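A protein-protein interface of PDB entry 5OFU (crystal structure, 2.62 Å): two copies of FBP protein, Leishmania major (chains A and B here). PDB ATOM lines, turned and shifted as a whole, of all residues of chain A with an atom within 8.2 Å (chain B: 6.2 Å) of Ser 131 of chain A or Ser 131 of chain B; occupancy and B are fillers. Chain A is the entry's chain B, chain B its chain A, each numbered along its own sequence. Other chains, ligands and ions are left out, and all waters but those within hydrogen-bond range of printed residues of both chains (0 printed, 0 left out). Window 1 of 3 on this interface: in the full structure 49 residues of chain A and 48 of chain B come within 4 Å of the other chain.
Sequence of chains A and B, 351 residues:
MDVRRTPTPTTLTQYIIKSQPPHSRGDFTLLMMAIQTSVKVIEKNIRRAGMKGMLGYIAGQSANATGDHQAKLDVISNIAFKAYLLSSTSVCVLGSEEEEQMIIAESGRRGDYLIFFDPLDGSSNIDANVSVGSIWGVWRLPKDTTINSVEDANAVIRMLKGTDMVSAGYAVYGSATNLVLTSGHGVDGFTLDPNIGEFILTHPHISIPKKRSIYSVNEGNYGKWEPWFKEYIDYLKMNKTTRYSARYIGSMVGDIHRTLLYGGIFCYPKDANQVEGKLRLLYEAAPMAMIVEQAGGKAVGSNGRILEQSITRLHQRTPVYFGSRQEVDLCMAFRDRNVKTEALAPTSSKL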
ATOM      1  N   ILE A  46     -12.670  -8.551 -11.816  1.00  0.00           N
ATOM      2  CA  ILE A  46     -11.842  -9.430 -12.627  1.00  0.00           C
ATOM      3  C   ILE A  46     -12.318  -9.480 -14.085  1.00  0.00           C
ATOM      4  O   ILE A  46     -11.487  -9.499 -15.006  1.00  0.00           O
ATOM      5  CB  ILE A  46     -11.747 -10.836 -12.003  1.00  0.00           C
ATOM      6  CG1 ILE A  46     -10.857 -10.757 -10.775  1.00  0.00           C
ATOM      7  CG2 ILE A  46     -11.152 -11.866 -12.965  1.00  0.00           C
ATOM      8  CD1 ILE A  46     -10.882 -12.017  -9.945  1.00  0.00           C
ATOM      9  N   LEU A 120      -7.241 -14.094  -4.242  1.00  0.00           N
ATOM     10  CA  LEU A 120      -6.955 -14.163  -5.682  1.00  0.00           C
ATOM     11  C   LEU A 120      -5.807 -15.126  -5.967  1.00  0.00           C
ATOM     12  O   LEU A 120      -4.641 -14.750  -6.072  1.00  0.00           O
ATOM     13  CB  LEU A 120      -6.693 -12.774  -6.267  1.00  0.00           C
ATOM     14  CG  LEU A 120      -6.736 -12.669  -7.799  1.00  0.00           C
ATOM     15  CD1 LEU A 120      -8.069 -13.130  -8.371  1.00  0.00           C
ATOM     16  CD2 LEU A 120      -6.468 -11.236  -8.235  1.00  0.00           C
ATOM     17  N   ASP A 121      -6.176 -16.398  -6.027  1.00  0.00           N
ATOM     18  CA  ASP A 121      -5.276 -17.495  -6.337  1.00  0.00           C
ATOM     19  C   ASP A 121      -4.977 -17.509  -7.832  1.00  0.00           C
ATOM     20  O   ASP A 121      -5.852 -17.242  -8.647  1.00  0.00           O
ATOM     21  CB  ASP A 121      -5.936 -18.818  -5.894  1.00  0.00           C
ATOM     22  CG  ASP A 121      -5.164 -20.041  -6.331  1.00  0.00           C
ATOM     23  OD1 ASP A 121      -4.174 -20.398  -5.646  1.00  0.00           O
ATOM     24  OD2 ASP A 121      -5.565 -20.630  -7.368  1.00  0.00           O
ATOM     25  N   GLY A 122      -3.739 -17.850  -8.168  1.00  0.00           N
ATOM     26  CA  GLY A 122      -3.279 -17.898  -9.547  1.00  0.00           C
ATOM     27  C   GLY A 122      -2.884 -16.529 -10.037  1.00  0.00           C
ATOM     28  O   GLY A 122      -3.145 -16.176 -11.183  1.00  0.00           O
ATOM     29  N   SER A 123      -2.200 -15.770  -9.183  1.00  0.00           N
ATOM     30  CA  SER A 123      -1.836 -14.369  -9.479  1.00  0.00           C
ATOM     31  C   SER A 123      -0.946 -14.178 -10.718  1.00  0.00           C
ATOM     32  O   SER A 123      -0.965 -13.110 -11.319  1.00  0.00           O
ATOM     33  CB  SER A 123      -1.169 -13.711  -8.263  1.00  0.00           C
ATOM     34  OG  SER A 123       0.110 -14.286  -8.020  1.00  0.00           O
ATOM     35  N   SER A 124      -0.171 -15.200 -11.089  1.00  0.00           N
ATOM     36  CA  SER A 124       0.638 -15.152 -12.315  1.00  0.00           C
ATOM     37  C   SER A 124      -0.211 -15.244 -13.600  1.00  0.00           C
ATOM     38  O   SER A 124       0.302 -14.930 -14.688  1.00  0.00           O
ATOM     39  CB  SER A 124       1.713 -16.249 -12.318  1.00  0.00           C
ATOM     40  OG  SER A 124       1.195 -17.476 -12.794  1.00  0.00           O
ATOM     41  N   ASN A 125      -1.477 -15.684 -13.471  1.00  0.00           N
ATOM     42  CA  ASN A 125      -2.446 -15.716 -14.588  1.00  0.00           C
ATOM     43  C   ASN A 125      -3.332 -14.458 -14.741  1.00  0.00           C
ATOM     44  O   ASN A 125      -4.145 -14.392 -15.673  1.00  0.00           O
ATOM     45  CB  ASN A 125      -3.337 -16.963 -14.492  1.00  0.00           C
ATOM     46  CG  ASN A 125      -2.634 -18.234 -14.950  1.00  0.00           C
ATOM     47  OD1 ASN A 125      -1.730 -18.213 -15.815  1.00  0.00           O
ATOM     48  ND2 ASN A 125      -3.066 -19.365 -14.403  1.00  0.00           N
ATOM     49  N   ILE A 126      -3.134 -13.449 -13.895  1.00  0.00           N
ATOM     50  CA  ILE A 126      -3.977 -12.257 -13.914  1.00  0.00           C
ATOM     51  C   ILE A 126      -3.818 -11.461 -15.217  1.00  0.00           C
ATOM     52  O   ILE A 126      -4.817 -11.114 -15.843  1.00  0.00           O
ATOM     53  CB  ILE A 126      -3.728 -11.339 -12.687  1.00  0.00           C
ATOM     54  CG1 ILE A 126      -4.160 -12.042 -11.402  1.00  0.00           C
ATOM     55  CG2 ILE A 126      -4.502 -10.028 -12.816  1.00  0.00           C
ATOM     56  CD1 ILE A 126      -3.618 -11.411 -10.131  1.00  0.00           C
ATOM     57  N   ALA A 128      -2.815 -12.268 -18.216  1.00  0.00           N
ATOM     58  CA  ALA A 128      -3.389 -12.983 -19.360  1.00  0.00           C
ATOM     59  C   ALA A 128      -4.915 -13.141 -19.282  1.00  0.00           C
ATOM     60  O   ALA A 128      -5.537 -13.582 -20.242  1.00  0.00           O
ATOM     61  CB  ALA A 128      -2.733 -14.344 -19.491  1.00  0.00           C
ATOM     62  N   ASN A 129      -5.511 -12.831 -18.128  1.00  0.00           N
ATOM     63  CA  ASN A 129      -6.947 -12.993 -17.892  1.00  0.00           C
ATOM     64  C   ASN A 129      -7.480 -14.402 -18.196  1.00  0.00           C
ATOM     65  O   ASN A 129      -8.583 -14.561 -18.727  1.00  0.00           O
ATOM     66  CB  ASN A 129      -7.737 -11.898 -18.642  1.00  0.00           C
ATOM     67  CG  ASN A 129      -7.931 -10.647 -17.802  1.00  0.00           C
ATOM     68  OD1 ASN A 129      -7.409  -9.584 -18.141  1.00  0.00           O
ATOM     69  ND2 ASN A 129      -8.652 -10.780 -16.678  1.00  0.00           N
ATOM     70  N   VAL A 130      -6.691 -15.416 -17.844  1.00  0.00           N
ATOM     71  CA  VAL A 130      -7.164 -16.801 -17.844  1.00  0.00           C
ATOM     72  C   VAL A 130      -7.679 -17.160 -16.428  1.00  0.00           C
ATOM     73  O   VAL A 130      -7.885 -16.263 -15.602  1.00  0.00           O
ATOM     74  CB  VAL A 130      -6.113 -17.756 -18.419  1.00  0.00           C
ATOM     75  CG1 VAL A 130      -5.742 -17.298 -19.823  1.00  0.00           C
ATOM     76  CG2 VAL A 130      -4.873 -17.868 -17.525  1.00  0.00           C
ATOM     77  N   SER A 131      -7.954 -18.433 -16.156  1.00  0.00           N
ATOM     78  CA  SER A 131      -8.680 -18.789 -14.935  1.00  0.00           C
ATOM     79  C   SER A 131      -7.902 -18.425 -13.677  1.00  0.00           C
ATOM     80  O   SER A 131      -6.705 -18.631 -13.610  1.00  0.00           O
ATOM     81  CB  SER A 131      -9.064 -20.263 -14.923  1.00  0.00           C
ATOM     82  OG  SER A 131     -10.074 -20.511 -15.888  1.00  0.00           O
ATOM     83  N   VAL A 132      -8.612 -17.829 -12.719  1.00  0.00           N
ATOM     84  CA  VAL A 132      -8.090 -17.504 -11.398  1.00  0.00           C
ATOM     85  C   VAL A 132      -9.188 -17.824 -10.385  1.00  0.00           C
ATOM     86  O   VAL A 132     -10.280 -18.248 -10.783  1.00  0.00           O
ATOM     87  CB  VAL A 132      -7.661 -16.025 -11.284  1.00  0.00           C
ATOM     88  CG1 VAL A 132      -6.342 -15.812 -11.993  1.00  0.00           C
ATOM     89  CG2 VAL A 132      -8.721 -15.081 -11.833  1.00  0.00           C
ATOM     90  N   GLY A 133      -8.908 -17.650  -9.092  1.00  0.00           N
ATOM     91  CA  GLY A 133      -9.877 -18.038  -8.085  1.00  0.00           C
ATOM     92  C   GLY A 133      -9.710 -17.465  -6.700  1.00  0.00           C
ATOM     93  O   GLY A 133      -8.763 -16.736  -6.435  1.00  0.00           O
ATOM     94  N   ALA A 171     -14.081 -20.242  -5.385  1.00  0.00           N
ATOM     95  CA  ALA A 171     -14.718 -19.652  -6.555  1.00  0.00           C
ATOM     96  C   ALA A 171     -13.711 -19.694  -7.701  1.00  0.00           C
ATOM     97  O   ALA A 171     -12.567 -19.281  -7.515  1.00  0.00           O
ATOM     98  CB  ALA A 171     -15.127 -18.215  -6.261  1.00  0.00           C
ATOM     99  N   VAL A 172     -14.121 -20.229  -8.846  1.00  0.00           N
ATOM    100  CA  VAL A 172     -13.306 -20.168 -10.079  1.00  0.00           C
ATOM    101  C   VAL A 172     -13.852 -19.086 -10.946  1.00  0.00           C
ATOM    102  O   VAL A 172     -15.020 -19.147 -11.325  1.00  0.00           O
ATOM    103  CB  VAL A 172     -13.362 -21.406 -10.995  1.00  0.00           C
ATOM    104  CG1 VAL A 172     -12.218 -21.385 -12.008  1.00  0.00           C
ATOM    105  CG2 VAL A 172     -13.229 -22.592 -10.126  1.00  0.00           C
ATOM    106  N   TYR A 173     -12.994 -18.139 -11.278  1.00  0.00           N
ATOM    107  CA  TYR A 173     -13.309 -17.104 -12.235  1.00  0.00           C
ATOM    108  C   TYR A 173     -12.717 -17.536 -13.580  1.00  0.00           C
ATOM    109  O   TYR A 173     -11.566 -17.227 -13.881  1.00  0.00           O
ATOM    110  CB  TYR A 173     -12.726 -15.779 -11.764  1.00  0.00           C
ATOM    111  CG  TYR A 173     -13.052 -15.451 -10.323  1.00  0.00           C
ATOM    112  CD1 TYR A 173     -14.360 -15.122  -9.935  1.00  0.00           C
ATOM    113  CD2 TYR A 173     -12.061 -15.449  -9.351  1.00  0.00           C
ATOM    114  CE1 TYR A 173     -14.656 -14.808  -8.616  1.00  0.00           C
ATOM    115  CE2 TYR A 173     -12.344 -15.149  -8.030  1.00  0.00           C
ATOM    116  CZ  TYR A 173     -13.643 -14.826  -7.662  1.00  0.00           C
ATOM    117  OH  TYR A 173     -13.925 -14.516  -6.351  1.00  0.00           O
ATOM    118  N   GLY A 174     -13.496 -18.310 -14.341  1.00  0.00           N
ATOM    119  CA  GLY A 174     -13.103 -18.797 -15.659  1.00  0.00           C
ATOM    120  C   GLY A 174     -13.991 -18.232 -16.755  1.00  0.00           C
ATOM    121  O   GLY A 174     -14.459 -17.081 -16.675  1.00  0.00           O
ATOM    122  N   SER A 175     -14.210 -19.035 -17.798  1.00  0.00           N
ATOM    123  CA  SER A 175     -15.124 -18.663 -18.879  1.00  0.00           C
ATOM    124  C   SER A 175     -16.558 -18.495 -18.351  1.00  0.00           C
ATOM    125  O   SER A 175     -17.333 -17.726 -18.901  1.00  0.00           O
ATOM    126  CB  SER A 175     -15.070 -19.685 -20.017  1.00  0.00           C
ATOM    127  OG  SER A 175     -15.609 -20.931 -19.628  1.00  0.00           O
ATOM    128  N   ALA A 176     -16.885 -19.239 -17.296  1.00  0.00           N
ATOM    129  CA  ALA A 176     -18.008 -18.952 -16.421  1.00  0.00           C
ATOM    130  C   ALA A 176     -17.481 -18.873 -14.994  1.00  0.00           C
ATOM    131  O   ALA A 176     -16.341 -19.257 -14.728  1.00  0.00           O
ATOM    132  CB  ALA A 176     -19.060 -20.042 -16.540  1.00  0.00           C
ATOM    133  N   ILE A 249      -2.982 -25.249 -15.824  1.00  0.00           N
ATOM    134  CA  ILE A 249      -3.395 -23.877 -16.004  1.00  0.00           C
ATOM    135  C   ILE A 249      -2.455 -22.908 -15.272  1.00  0.00           C
ATOM    136  O   ILE A 249      -2.167 -21.831 -15.789  1.00  0.00           O
ATOM    137  CB  ILE A 249      -4.851 -23.687 -15.517  1.00  0.00           C
ATOM    138  CG1 ILE A 249      -5.819 -24.511 -16.379  1.00  0.00           C
ATOM    139  CG2 ILE A 249      -5.260 -22.214 -15.534  1.00  0.00           C
ATOM    140  CD1 ILE A 249      -7.187 -24.680 -15.767  1.00  0.00           C
ATOM    141  N   GLY A 250      -1.969 -23.289 -14.085  1.00  0.00           N
ATOM    142  CA  GLY A 250      -1.130 -22.411 -13.251  1.00  0.00           C
ATOM    143  C   GLY A 250      -1.885 -21.710 -12.133  1.00  0.00           C
ATOM    144  O   GLY A 250      -1.307 -20.888 -11.410  1.00  0.00           O
ATOM    145  N   SER A 251      -3.183 -21.989 -12.029  1.00  0.00           N
ATOM    146  CA  SER A 251      -3.990 -21.563 -10.902  1.00  0.00           C
ATOM    147  C   SER A 251      -4.526 -22.817 -10.248  1.00  0.00           C
ATOM    148  O   SER A 251      -5.225 -23.598 -10.893  1.00  0.00           O
ATOM    149  CB  SER A 251      -5.147 -20.667 -11.365  1.00  0.00           C
ATOM    150  OG  SER A 251      -4.645 -19.598 -12.170  1.00  0.00           O
ATOM    151  N   MET A 252      -4.202 -22.994  -8.970  1.00  0.00           N
ATOM    152  CA  MET A 252      -4.633 -24.162  -8.211  1.00  0.00           C
ATOM    153  C   MET A 252      -6.152 -24.362  -8.279  1.00  0.00           C
ATOM    154  O   MET A 252      -6.626 -25.484  -8.419  1.00  0.00           O
ATOM    155  CB  MET A 252      -4.181 -24.047  -6.755  1.00  0.00           C
ATOM    156  CG  MET A 252      -4.434 -25.305  -5.949  1.00  0.00           C
ATOM    157  SD  MET A 252      -4.482 -25.038  -4.172  1.00  0.00           S
ATOM    158  CE  MET A 252      -4.520 -26.740  -3.583  1.00  0.00           C
ATOM    159  N   VAL A 253      -6.908 -23.270  -8.192  1.00  0.00           N
ATOM    160  CA  VAL A 253      -8.365 -23.345  -8.199  1.00  0.00           C
ATOM    161  C   VAL A 253      -8.858 -23.833  -9.556  1.00  0.00           C
ATOM    162  O   VAL A 253      -9.750 -24.666  -9.616  1.00  0.00           O
ATOM    163  CB  VAL A 253      -9.015 -22.000  -7.809  1.00  0.00           C
ATOM    164  CG1 VAL A 253     -10.530 -22.080  -7.923  1.00  0.00           C
ATOM    165  CG2 VAL A 253      -8.656 -21.629  -6.378  1.00  0.00           C
ATOM    166  N   GLY A 254      -8.269 -23.322 -10.632  1.00  0.00           N
ATOM    167  CA  GLY A 254      -8.589 -23.796 -11.971  1.00  0.00           C
ATOM    168  C   GLY A 254      -8.272 -25.264 -12.174  1.00  0.00           C
ATOM    169  O   GLY A 254      -9.111 -26.029 -12.644  1.00  0.00           O
ATOM    170  N   ASP A 255      -7.062 -25.665 -11.800  1.00  0.00           N
ATOM    171  CA  ASP A 255      -6.615 -27.065 -11.973  1.00  0.00           C
ATOM    172  C   ASP A 255      -7.412 -28.063 -11.119  1.00  0.00           C
ATOM    173  O   ASP A 255      -7.838 -29.105 -11.623  1.00  0.00           O
ATOM    174  CB  ASP A 255      -5.118 -27.192 -11.694  1.00  0.00           C
ATOM    175  CG  ASP A 255      -4.251 -26.489 -12.757  1.00  0.00           C
ATOM    176  OD1 ASP A 255      -4.464 -26.749 -13.967  1.00  0.00           O
ATOM    177  OD2 ASP A 255      -3.332 -25.709 -12.377  1.00  0.00           O
ATOM    178  N   HIS A 257     -10.493 -27.555  -9.902  1.00  0.00           N
ATOM    179  CA  HIS A 257     -11.848 -27.570 -10.427  1.00  0.00           C
ATOM    180  C   HIS A 257     -12.011 -28.527 -11.611  1.00  0.00           C
ATOM    181  O   HIS A 257     -12.953 -29.314 -11.647  1.00  0.00           O
ATOM    182  CB  HIS A 257     -12.289 -26.166 -10.807  1.00  0.00           C
ATOM    183  CG  HIS A 257     -13.695 -26.094 -11.288  1.00  0.00           C
ATOM    184  ND1 HIS A 257     -14.777 -26.360 -10.477  1.00  0.00           N
ATOM    185  CD2 HIS A 257     -14.197 -25.788 -12.501  1.00  0.00           C
ATOM    186  CE1 HIS A 257     -15.889 -26.211 -11.172  1.00  0.00           C
ATOM    187  NE2 HIS A 257     -15.564 -25.863 -12.405  1.00  0.00           N
ATOM    188  N   ASP B 121     -12.798 -23.185 -29.752  1.00  0.00           N
ATOM    189  CA  ASP B 121     -11.526 -23.835 -29.520  1.00  0.00           C
ATOM    190  C   ASP B 121     -11.358 -24.191 -28.048  1.00  0.00           C
ATOM    191  O   ASP B 121     -11.751 -23.426 -27.170  1.00  0.00           O
ATOM    192  CB  ASP B 121     -10.404 -22.897 -29.975  1.00  0.00           C
ATOM    193  CG  ASP B 121      -9.028 -23.408 -29.634  1.00  0.00           C
ATOM    194  OD1 ASP B 121      -8.497 -24.267 -30.384  1.00  0.00           O
ATOM    195  OD2 ASP B 121      -8.462 -22.929 -28.625  1.00  0.00           O
ATOM    196  N   GLY B 122     -10.734 -25.343 -27.798  1.00  0.00           N
ATOM    197  CA  GLY B 122     -10.497 -25.845 -26.444  1.00  0.00           C
ATOM    198  C   GLY B 122     -11.717 -26.556 -25.901  1.00  0.00           C
ATOM    199  O   GLY B 122     -12.061 -26.394 -24.738  1.00  0.00           O
ATOM    200  N   ASN B 125     -12.033 -28.227 -22.534  1.00  0.00           N
ATOM    201  CA  ASN B 125     -12.141 -27.324 -21.366  1.00  0.00           C
ATOM    202  C   ASN B 125     -13.552 -26.736 -21.098  1.00  0.00           C
ATOM    203  O   ASN B 125     -13.729 -25.986 -20.126  1.00  0.00           O
ATOM    204  CB  ASN B 125     -11.119 -26.183 -21.469  1.00  0.00           C
ATOM    205  CG  ASN B 125      -9.706 -26.610 -21.097  1.00  0.00           C
ATOM    206  OD1 ASN B 125      -9.487 -27.528 -20.295  1.00  0.00           O
ATOM    207  ND2 ASN B 125      -8.728 -25.927 -21.671  1.00  0.00           N
ATOM    208  N   ASN B 129     -15.370 -25.087 -17.549  1.00  0.00           N
ATOM    209  CA  ASN B 129     -15.545 -23.645 -17.703  1.00  0.00           C
ATOM    210  C   ASN B 129     -14.276 -22.833 -17.435  1.00  0.00           C
ATOM    211  O   ASN B 129     -14.325 -21.742 -16.858  1.00  0.00           O
ATOM    212  CB  ASN B 129     -16.741 -23.146 -16.867  1.00  0.00           C
ATOM    213  CG  ASN B 129     -18.044 -23.195 -17.641  1.00  0.00           C
ATOM    214  OD1 ASN B 129     -18.962 -23.931 -17.269  1.00  0.00           O
ATOM    215  ND2 ASN B 129     -18.136 -22.404 -18.728  1.00  0.00           N
ATOM    216  N   VAL B 130     -13.144 -23.367 -17.881  1.00  0.00           N
ATOM    217  CA  VAL B 130     -11.899 -22.602 -17.921  1.00  0.00           C
ATOM    218  C   VAL B 130     -11.741 -21.956 -19.323  1.00  0.00           C
ATOM    219  O   VAL B 130     -12.702 -21.922 -20.095  1.00  0.00           O
ATOM    220  CB  VAL B 130     -10.702 -23.454 -17.450  1.00  0.00           C
ATOM    221  CG1 VAL B 130     -10.981 -23.975 -16.041  1.00  0.00           C
ATOM    222  CG2 VAL B 130     -10.382 -24.603 -18.410  1.00  0.00           C
ATOM    223  N   SER B 131     -10.569 -21.406 -19.644  1.00  0.00           N
ATOM    224  CA  SER B 131     -10.442 -20.575 -20.846  1.00  0.00           C
ATOM    225  C   SER B 131     -10.700 -21.358 -22.128  1.00  0.00           C
ATOM    226  O   SER B 131     -10.266 -22.491 -22.260  1.00  0.00           O
ATOM    227  CB  SER B 131      -9.083 -19.896 -20.913  1.00  0.00           C
ATOM    228  OG  SER B 131      -9.001 -18.894 -19.915  1.00  0.00           O
ATOM    229  N   VAL B 132     -11.490 -20.757 -23.012  1.00  0.00           N
ATOM    230  CA  VAL B 132     -11.794 -21.288 -24.337  1.00  0.00           C
ATOM    231  C   VAL B 132     -11.804 -20.096 -25.305  1.00  0.00           C
ATOM    232  O   VAL B 132     -11.581 -18.961 -24.882  1.00  0.00           O
ATOM    233  CB  VAL B 132     -13.153 -22.026 -24.388  1.00  0.00           C
ATOM    234  CG1 VAL B 132     -13.035 -23.388 -23.744  1.00  0.00           C
ATOM    235  CG2 VAL B 132     -14.271 -21.208 -23.738  1.00  0.00           C
ATOM    236  N   GLY B 133     -12.012 -20.351 -26.595  1.00  0.00           N
ATOM    237  CA  GLY B 133     -11.874 -19.289 -27.580  1.00  0.00           C
ATOM    238  C   GLY B 133     -12.476 -19.530 -28.933  1.00  0.00           C
ATOM    239  O   GLY B 133     -12.999 -20.603 -29.208  1.00  0.00           O
ATOM    240  N   VAL B 172     -10.570 -14.717 -26.761  1.00  0.00           N
ATOM    241  CA  VAL B 172     -10.326 -15.571 -25.581  1.00  0.00           C
ATOM    242  C   VAL B 172     -11.433 -15.302 -24.574  1.00  0.00           C
ATOM    243  O   VAL B 172     -11.666 -14.155 -24.159  1.00  0.00           O
ATOM    244  CB  VAL B 172      -8.901 -15.386 -25.002  1.00  0.00           C
ATOM    245  CG1 VAL B 172      -8.567 -13.941 -24.719  1.00  0.00           C
ATOM    246  CG2 VAL B 172      -8.670 -16.202 -23.741  1.00  0.00           C
ATOM    247  N   TYR B 173     -12.184 -16.354 -24.258  1.00  0.00           N
ATOM    248  CA  TYR B 173     -13.224 -16.301 -23.232  1.00  0.00           C
ATOM    249  C   TYR B 173     -12.592 -16.847 -21.950  1.00  0.00           C
ATOM    250  O   TYR B 173     -12.641 -18.043 -21.681  1.00  0.00           O
ATOM    251  CB  TYR B 173     -14.439 -17.129 -23.657  1.00  0.00           C
ATOM    252  CG  TYR B 173     -14.928 -16.826 -25.059  1.00  0.00           C
ATOM    253  CD1 TYR B 173     -15.529 -15.610 -25.370  1.00  0.00           C
ATOM    254  CD2 TYR B 173     -14.789 -17.764 -26.073  1.00  0.00           C
ATOM    255  CE1 TYR B 173     -15.986 -15.338 -26.657  1.00  0.00           C
ATOM    256  CE2 TYR B 173     -15.224 -17.501 -27.365  1.00  0.00           C
ATOM    257  CZ  TYR B 173     -15.824 -16.288 -27.651  1.00  0.00           C
ATOM    258  OH  TYR B 173     -16.266 -16.039 -28.932  1.00  0.00           O
ATOM    259  N   GLY B 174     -11.965 -15.951 -21.192  1.00  0.00           N
ATOM    260  CA  GLY B 174     -11.333 -16.284 -19.913  1.00  0.00           C
ATOM    261  C   GLY B 174     -11.990 -15.597 -18.721  1.00  0.00           C
ATOM    262  O   GLY B 174     -13.202 -15.364 -18.713  1.00  0.00           O
ATOM    263  N   SER B 175     -11.174 -15.248 -17.727  1.00  0.00           N
ATOM    264  CA  SER B 175     -11.633 -14.465 -16.589  1.00  0.00           C
ATOM    265  C   SER B 175     -12.133 -13.087 -17.027  1.00  0.00           C
ATOM    266  O   SER B 175     -13.001 -12.511 -16.383  1.00  0.00           O
ATOM    267  CB  SER B 175     -10.525 -14.335 -15.538  1.00  0.00           C
ATOM    268  OG  SER B 175      -9.452 -13.527 -15.989  1.00  0.00           O
ATOM    269  N   ILE B 249      -2.889 -24.831 -20.570  1.00  0.00           N
ATOM    270  CA  ILE B 249      -4.309 -24.724 -20.298  1.00  0.00           C
ATOM    271  C   ILE B 249      -5.089 -25.824 -21.022  1.00  0.00           C
ATOM    272  O   ILE B 249      -6.047 -26.333 -20.482  1.00  0.00           O
ATOM    273  CB  ILE B 249      -4.833 -23.315 -20.697  1.00  0.00           C
ATOM    274  CG1 ILE B 249      -4.181 -22.221 -19.827  1.00  0.00           C
ATOM    275  CG2 ILE B 249      -6.353 -23.225 -20.591  1.00  0.00           C
ATOM    276  CD1 ILE B 249      -4.339 -20.814 -20.380  1.00  0.00           C
ATOM    277  N   GLY B 250      -4.679 -26.174 -22.236  1.00  0.00           N
ATOM    278  CA  GLY B 250      -5.420 -27.130 -23.080  1.00  0.00           C
ATOM    279  C   GLY B 250      -6.331 -26.490 -24.131  1.00  0.00           C
ATOM    280  O   GLY B 250      -7.053 -27.195 -24.838  1.00  0.00           O
ATOM    281  N   SER B 251      -6.346 -25.159 -24.185  1.00  0.00           N
ATOM    282  CA  SER B 251      -7.006 -24.409 -25.242  1.00  0.00           C
ATOM    283  C   SER B 251      -5.934 -23.586 -25.920  1.00  0.00           C
ATOM    284  O   SER B 251      -5.275 -22.767 -25.275  1.00  0.00           O
ATOM    285  CB  SER B 251      -8.091 -23.497 -24.678  1.00  0.00           C
ATOM    286  OG  SER B 251      -8.975 -24.239 -23.848  1.00  0.00           O
ATOM    287  N   GLY B 254      -6.222 -19.840 -25.370  1.00  0.00           N
ATOM    288  CA  GLY B 254      -5.733 -19.480 -24.039  1.00  0.00           C
ATOM    289  C   GLY B 254      -4.213 -19.477 -23.933  1.00  0.00           C
ATOM    290  O   GLY B 254      -3.627 -18.513 -23.463  1.00  0.00           O
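The backbone carbonyl oxygen of Val 130 of chain A lies within hydrogen-bond range of the side-chain hydroxyl of Ser 175 of chain B, 3.2 Å away.
The backbone carbonyl oxygen (O) of Gly 174 of chain A lies close to the backbone carbonyl oxygen (O) of Gly 174 of chain B (2.9 Å).
N of Ser 175 of chain B lies within hydrogen-bond range of O of Asn 129 of chain A (2.9 Å).
The backbone carbonyl oxygen of Val 130 of chain B is in hydrogen-bond range of the side-chain hydroxyl of Ser 175 of chain A (3.1 Å).
The backbone NH (N) of Ser 175 of chain A sits at hydrogen-bond distance from the backbone carbonyl oxygen (O) of Asn 129 of chain B.
O of Ser 131 of chain A lies within hydrogen-bond range of OG of Ser 251 of chain A (2.7 Å).
The backbone NH (N) of Val 130 of chain B is in hydrogen-bond range of the backbone carbonyl oxygen (O) of Asn 125 of chain B (3.5 Å).
The side-chain carboxylate (OD1) of Asp 255 of chain A sits at hydrogen-bond distance from the backbone NH (N) of Ile 249 of chain A, at 2.8 Å.
O of Val 132 of chain A is in hydrogen-bond range of N of Tyr 173 of chain A (2.8 Å).
The backbone carbonyl oxygen (O) of Val 132 of chain B lies within hydrogen-bond range of the backbone NH (N) of Tyr 173 of chain B, 2.7 Å away.
Among the printed residues, merely in contact across the chains: Ile 46 of chain A with Ser 175 of chain B (3.6 Å), Asn 129 of chain A with Gly 174 of chain B (3.5 Å), Val 130 of chain A with Ser 131 of chain B (3.4 Å), Val 130 of chain A with Ile 249 of chain B (3.8 Å), Ser 131 of chain A with Val 130 of chain B (3.4 Å), Ser 131 of chain A with Ser 131 of chain B (3.9 Å), Tyr 173 of chain A with Ser 175 of chain B (3.5 Å), Gly 174 of chain A with Asn 129 of chain B (3.4 Å), Gly 174 of chain A with Ser 175 of chain B (3.9 Å), Ser 175 of chain A with Tyr 173 of chain B (3.4 Å), Ser 175 of chain A with Gly 174 of chain B (3.8 Å), Ala 176 of chain A with Asn 129 of chain B (3.3 Å) and Ile 249 of chain A with Val 130 of chain B (3.9 Å).
Of the printed residues of chain B, Ser 175 of chain A touches Asn 129 (2.9 Å), Val 130 (3.1 Å), Tyr 173 (3.4 Å) and Gly 174 (3.8 Å).
Printed residues of chain B within 4 Å of Ile 249 of chain A: Val 130 (3.9 Å).
Of the printed residues of chain A, Asn 129 of chain B touches Gly 174, Ser 175 and Ala 176.
Val 130 of chain B touches just these residues of chain A: Ser 131, Ser 175 and Ile 249.
Ser 131 of chain B touches just these residues of chain A: Val 130 (3.4 Å) and Ser 131 (3.9 Å).
No residue of chain A comes within 4 Å of Val 132 of chain B.
Of the printed residues of chain A, Gly 174 of chain B touches Asn 129 (3.5 Å), Gly 174 (2.9 Å) and Ser 175 (3.8 Å).
Printed residues of chain A within 4 Å of Ser 175 of chain B: Ile 46 (3.6 Å), Asn 129 (2.9 Å), Val 130 (3.2 Å), Tyr 173 (3.5 Å) and Gly 174 (3.9 Å).
The nearest residue of chain B that does not touch Ser 131 of chain A is Asn 129 of chain B (4.5 Å).
Of the 16 printed residues of chain B, 7 touch a printed residue of chain A.
Hydrophobic or aromatic side chains of chain B that line the printed part of chain A: Val 130 and Ile 249.
Asn 129 of chain A touches Gly 174 of chain B, and with the chains exchanged Gly 174 of chain A touches Asn 129 of chain B.
Asn 129 of chain A touches Ser 175 of chain B, and with the chains exchanged Ser 175 of chain A touches Asn 129 of chain B.
Val 130 of chain A touches Ile 249 of chain B, and with the chains exchanged Ile 249 of chain A touches Val 130 of chain B.
Positions printed for both chains: 121, 122, 125, 129, 130, 131, 132, 133, 172, 173, 174, 175, 249, 250, 251 and 254.
Of the 18 pairs that touch across the chains among the printed residues, 16 have their exchanged pair printed and touching as well.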
